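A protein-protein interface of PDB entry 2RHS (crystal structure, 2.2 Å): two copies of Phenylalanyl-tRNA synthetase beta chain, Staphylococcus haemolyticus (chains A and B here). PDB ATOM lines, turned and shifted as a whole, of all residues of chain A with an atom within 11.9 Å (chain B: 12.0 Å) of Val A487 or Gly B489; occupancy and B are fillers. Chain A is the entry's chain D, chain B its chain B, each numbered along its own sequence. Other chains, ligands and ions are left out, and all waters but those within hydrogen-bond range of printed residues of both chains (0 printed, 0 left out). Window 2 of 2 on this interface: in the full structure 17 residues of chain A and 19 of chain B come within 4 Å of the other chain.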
ATOM      1  N   SER A 483      27.597  38.070  -1.582  1.00  0.00           N
ATOM      2  CA  SER A 483      26.278  37.691  -2.076  1.00  0.00           C
ATOM      3  C   SER A 483      26.015  36.223  -1.784  1.00  0.00           C
ATOM      4  O   SER A 483      26.820  35.354  -2.121  1.00  0.00           O
ATOM      5  CB  SER A 483      26.192  37.942  -3.577  1.00  0.00           C
ATOM      6  OG  SER A 483      25.067  37.268  -4.090  1.00  0.00           O
ATOM      7  N   SER A 484      24.889  35.950  -1.137  1.00  0.00           N
ATOM      8  CA  SER A 484      24.587  34.591  -0.716  1.00  0.00           C
ATOM      9  C   SER A 484      23.089  34.342  -0.871  1.00  0.00           C
ATOM     10  O   SER A 484      22.330  35.268  -1.147  1.00  0.00           O
ATOM     11  CB  SER A 484      25.063  34.365   0.719  1.00  0.00           C
ATOM     12  OG  SER A 484      24.131  34.908   1.632  1.00  0.00           O
ATOM     13  N   LEU A 485      22.649  33.101  -0.712  1.00  0.00           N
ATOM     14  CA  LEU A 485      21.219  32.803  -0.795  1.00  0.00           C
ATOM     15  C   LEU A 485      20.763  32.070   0.458  1.00  0.00           C
ATOM     16  O   LEU A 485      21.453  31.199   0.957  1.00  0.00           O
ATOM     17  CB  LEU A 485      20.899  31.982  -2.056  1.00  0.00           C
ATOM     18  CG  LEU A 485      20.817  32.803  -3.347  1.00  0.00           C
ATOM     19  CD1 LEU A 485      21.098  31.918  -4.556  1.00  0.00           C
ATOM     20  CD2 LEU A 485      19.455  33.497  -3.494  1.00  0.00           C
ATOM     21  N   PRO A 486      19.581  32.412   0.969  1.00  0.00           N
ATOM     22  CA  PRO A 486      19.145  31.766   2.186  1.00  0.00           C
ATOM     23  C   PRO A 486      18.799  30.279   2.024  1.00  0.00           C
ATOM     24  O   PRO A 486      18.122  29.855   1.066  1.00  0.00           O
ATOM     25  CB  PRO A 486      17.931  32.591   2.607  1.00  0.00           C
ATOM     26  CG  PRO A 486      17.483  33.324   1.434  1.00  0.00           C
ATOM     27  CD  PRO A 486      18.605  33.386   0.449  1.00  0.00           C
ATOM     28  N   VAL A 487      19.299  29.495   2.980  1.00  0.00           N
ATOM     29  CA  VAL A 487      19.095  28.047   2.987  1.00  0.00           C
ATOM     30  C   VAL A 487      18.118  27.645   4.083  1.00  0.00           C
ATOM     31  O   VAL A 487      18.414  27.767   5.271  1.00  0.00           O
ATOM     32  CB  VAL A 487      20.399  27.281   3.248  1.00  0.00           C
ATOM     33  CG1 VAL A 487      20.090  25.794   3.306  1.00  0.00           C
ATOM     34  CG2 VAL A 487      21.445  27.580   2.176  1.00  0.00           C
ATOM     35  N   PHE A 488      16.961  27.153   3.661  1.00  0.00           N
ATOM     36  CA  PHE A 488      15.787  26.983   4.498  1.00  0.00           C
ATOM     37  C   PHE A 488      15.733  25.547   5.008  1.00  0.00           C
ATOM     38  O   PHE A 488      15.767  24.579   4.243  1.00  0.00           O
ATOM     39  CB  PHE A 488      14.557  27.253   3.630  1.00  0.00           C
ATOM     40  CG  PHE A 488      14.405  28.698   3.223  1.00  0.00           C
ATOM     41  CD1 PHE A 488      14.155  29.680   4.173  1.00  0.00           C
ATOM     42  CD2 PHE A 488      14.504  29.074   1.888  1.00  0.00           C
ATOM     43  CE1 PHE A 488      14.010  31.011   3.801  1.00  0.00           C
ATOM     44  CE2 PHE A 488      14.359  30.412   1.505  1.00  0.00           C
ATOM     45  CZ  PHE A 488      14.115  31.374   2.461  1.00  0.00           C
ATOM     46  N   GLY A 489      15.653  25.417   6.325  1.00  0.00           N
ATOM     47  CA  GLY A 489      15.848  24.126   6.953  1.00  0.00           C
ATOM     48  C   GLY A 489      14.505  23.441   7.091  1.00  0.00           C
ATOM     49  O   GLY A 489      14.451  22.229   7.137  1.00  0.00           O
ATOM     50  N   GLU A 490      13.420  24.203   7.180  1.00  0.00           N
ATOM     51  CA  GLU A 490      12.103  23.646   6.896  1.00  0.00           C
ATOM     52  C   GLU A 490      11.955  23.602   5.372  1.00  0.00           C
ATOM     53  O   GLU A 490      11.861  24.634   4.688  1.00  0.00           O
ATOM     54  CB  GLU A 490      11.002  24.476   7.555  1.00  0.00           C
ATOM     55  CG  GLU A 490       9.870  23.699   8.213  1.00  0.00           C
ATOM     56  CD  GLU A 490       9.304  24.429   9.437  1.00  0.00           C
ATOM     57  OE1 GLU A 490       9.891  24.319  10.540  1.00  0.00           O
ATOM     58  OE2 GLU A 490       8.265  25.123   9.304  1.00  0.00           O
ATOM     59  N   VAL A 491      11.974  22.391   4.827  1.00  0.00           N
ATOM     60  CA  VAL A 491      11.935  22.285   3.376  1.00  0.00           C
ATOM     61  C   VAL A 491      10.492  22.088   2.949  1.00  0.00           C
ATOM     62  O   VAL A 491       9.730  21.340   3.561  1.00  0.00           O
ATOM     63  CB  VAL A 491      12.804  21.159   2.814  1.00  0.00           C
ATOM     64  CG1 VAL A 491      12.726  21.177   1.316  1.00  0.00           C
ATOM     65  CG2 VAL A 491      14.249  21.331   3.258  1.00  0.00           C
ATOM     66  N   THR A 492      10.137  22.805   1.894  1.00  0.00           N
ATOM     67  CA  THR A 492       8.763  22.944   1.467  1.00  0.00           C
ATOM     68  C   THR A 492       8.895  23.251  -0.025  1.00  0.00           C
ATOM     69  O   THR A 492       9.778  24.001  -0.468  1.00  0.00           O
ATOM     70  CB  THR A 492       8.034  24.035   2.306  1.00  0.00           C
ATOM     71  OG1 THR A 492       6.630  23.761   2.380  1.00  0.00           O
ATOM     72  CG2 THR A 492       8.236  25.422   1.749  1.00  0.00           C
ATOM     73  N   LEU B 485      13.466  15.765   4.442  1.00  0.00           N
ATOM     74  CA  LEU B 485      13.713  16.272   3.105  1.00  0.00           C
ATOM     75  C   LEU B 485      15.081  16.889   3.003  1.00  0.00           C
ATOM     76  O   LEU B 485      15.465  17.658   3.885  1.00  0.00           O
ATOM     77  CB  LEU B 485      12.689  17.329   2.703  1.00  0.00           C
ATOM     78  CG  LEU B 485      11.291  16.764   2.521  1.00  0.00           C
ATOM     79  CD1 LEU B 485      10.324  17.913   2.732  1.00  0.00           C
ATOM     80  CD2 LEU B 485      11.237  16.197   1.116  1.00  0.00           C
ATOM     81  N   PRO B 486      15.788  16.592   1.900  1.00  0.00           N
ATOM     82  CA  PRO B 486      17.177  17.023   1.799  1.00  0.00           C
ATOM     83  C   PRO B 486      17.203  18.538   1.614  1.00  0.00           C
ATOM     84  O   PRO B 486      16.349  19.071   0.908  1.00  0.00           O
ATOM     85  CB  PRO B 486      17.679  16.334   0.519  1.00  0.00           C
ATOM     86  CG  PRO B 486      16.410  16.101  -0.358  1.00  0.00           C
ATOM     87  CD  PRO B 486      15.313  15.877   0.696  1.00  0.00           C
ATOM     88  N   VAL B 487      18.184  19.194   2.236  1.00  0.00           N
ATOM     89  CA  VAL B 487      18.333  20.639   2.280  1.00  0.00           C
ATOM     90  C   VAL B 487      19.599  20.859   1.482  1.00  0.00           C
ATOM     91  O   VAL B 487      20.671  20.383   1.835  1.00  0.00           O
ATOM     92  CB  VAL B 487      18.523  21.142   3.728  1.00  0.00           C
ATOM     93  CG1 VAL B 487      18.629  22.670   3.806  1.00  0.00           C
ATOM     94  CG2 VAL B 487      17.369  20.689   4.596  1.00  0.00           C
ATOM     95  N   PHE B 488      19.470  21.579   0.380  1.00  0.00           N
ATOM     96  CA  PHE B 488      20.578  21.811  -0.508  1.00  0.00           C
ATOM     97  C   PHE B 488      21.236  23.140  -0.116  1.00  0.00           C
ATOM     98  O   PHE B 488      20.579  24.186  -0.054  1.00  0.00           O
ATOM     99  CB  PHE B 488      20.046  21.828  -1.939  1.00  0.00           C
ATOM    100  CG  PHE B 488      19.332  20.558  -2.327  1.00  0.00           C
ATOM    101  CD1 PHE B 488      20.036  19.366  -2.488  1.00  0.00           C
ATOM    102  CD2 PHE B 488      17.971  20.558  -2.545  1.00  0.00           C
ATOM    103  CE1 PHE B 488      19.399  18.198  -2.850  1.00  0.00           C
ATOM    104  CE2 PHE B 488      17.313  19.384  -2.911  1.00  0.00           C
ATOM    105  CZ  PHE B 488      18.030  18.206  -3.069  1.00  0.00           C
ATOM    106  N   GLY B 489      22.536  23.074   0.163  1.00  0.00           N
ATOM    107  CA  GLY B 489      23.301  24.193   0.696  1.00  0.00           C
ATOM    108  C   GLY B 489      23.638  25.046  -0.503  1.00  0.00           C
ATOM    109  O   GLY B 489      23.847  26.257  -0.384  1.00  0.00           O
ATOM    110  N   GLU B 490      23.669  24.407  -1.668  1.00  0.00           N
ATOM    111  CA  GLU B 490      23.758  25.147  -2.913  1.00  0.00           C
ATOM    112  C   GLU B 490      22.386  25.460  -3.529  1.00  0.00           C
ATOM    113  O   GLU B 490      21.650  24.584  -4.012  1.00  0.00           O
ATOM    114  CB  GLU B 490      24.687  24.431  -3.889  1.00  0.00           C
ATOM    115  CG  GLU B 490      24.205  24.502  -5.340  1.00  0.00           C
ATOM    116  CD  GLU B 490      25.019  25.474  -6.162  1.00  0.00           C
ATOM    117  OE1 GLU B 490      25.570  26.424  -5.556  1.00  0.00           O
ATOM    118  OE2 GLU B 490      25.106  25.283  -7.396  1.00  0.00           O
ATOM    119  N   VAL B 491      22.033  26.738  -3.502  1.00  0.00           N
ATOM    120  CA  VAL B 491      20.640  27.138  -3.644  1.00  0.00           C
ATOM    121  C   VAL B 491      20.353  27.605  -5.061  1.00  0.00           C
ATOM    122  O   VAL B 491      21.094  28.425  -5.598  1.00  0.00           O
ATOM    123  CB  VAL B 491      20.278  28.233  -2.635  1.00  0.00           C
ATOM    124  CG1 VAL B 491      18.818  28.634  -2.794  1.00  0.00           C
ATOM    125  CG2 VAL B 491      20.526  27.725  -1.248  1.00  0.00           C
ATOM    126  N   THR B 492      19.288  27.079  -5.658  1.00  0.00           N
ATOM    127  CA  THR B 492      18.891  27.417  -7.021  1.00  0.00           C
ATOM    128  C   THR B 492      17.377  27.467  -7.086  1.00  0.00           C
ATOM    129  O   THR B 492      16.674  26.755  -6.374  1.00  0.00           O
ATOM    130  CB  THR B 492      19.320  26.350  -8.053  1.00  0.00           C
ATOM    131  OG1 THR B 492      18.964  25.058  -7.551  1.00  0.00           O
ATOM    132  CG2 THR B 492      20.815  26.409  -8.337  1.00  0.00           C
ATOM    133  N   SER B 493      16.872  28.331  -7.955  1.00  0.00           N
ATOM    134  CA  SER B 493      15.454  28.340  -8.242  1.00  0.00           C
ATOM    135  C   SER B 493      15.172  27.236  -9.248  1.00  0.00           C
ATOM    136  O   SER B 493      15.820  27.142 -10.292  1.00  0.00           O
ATOM    137  CB  SER B 493      15.037  29.702  -8.781  1.00  0.00           C
ATOM    138  OG  SER B 493      13.663  29.654  -9.118  1.00  0.00           O
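Printed residues of chain A that touch a printed residue of chain B: Leu A485, Pro A486, Val A487, Phe A488 and Val A491. Among the printed residues, no Asp or Glu carboxylate lies within 4 Å of a Lys or Arg side-chain nitrogen of the other chain.
Val B491 touches Leu A485 (O to CD1, 3.6 Å). Pro A486 touches Val B491 (O to CG2, 3.96 Å). Val A487 touches Val B487. Phe B488 touches Val A487 (O to CG1, 3.8 Å). CG2 of Val A487 touches O of Gly B489 (3.8 Å). Val A487 touches Val B491 (CG2 to CG2, 3.5 Å). Val B487 touches Phe A488. Leu B485 touches Val A491 (CD1 to O, 3.6 Å). CG2 of Val A491 touches O of Pro B486, 3.9 Å away. Val B487 touches Val A491 (CG2 to CG2, 3.5 Å).
Leu A485 touches Val B491, and with the chains exchanged Val A491 touches Leu B485. Pro A486 touches Val B491, and with the chains exchanged Val A491 touches Pro B486. Val B487 touches its own counterpart, Val A487. Val A487 touches Val B491, and with the chains exchanged Val A491 touches Val B487.
Val A487 touches just these residues of chain B: Val B487, Phe B488, Gly B489 and Val B491. Gly B489 touches just one residue of chain A: Val A487. Leu A485 touches just one residue of chain B: Val B491. No residue of chain B comes within 4 Å of Gly A489. No residue of chain A comes within 4 Å of Glu B490. Val B491 touches just these residues of chain A: Leu A485, Pro A486 and Val A487. Of the printed residues of chain A, Pro B486 touches Val A491 (3.9 Å). Printed residues of chain B within 4 Å of Val A491: Leu B485, Pro B486 and Val B487. Glu A490 touches none of the printed residues of chain B. The nearest residue of chain B that does not touch Val A487 is Glu B490 (5.5 Å). The nearest printed residue of chain B that does not touch Val A491 is Phe B488 (6.0 Å).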
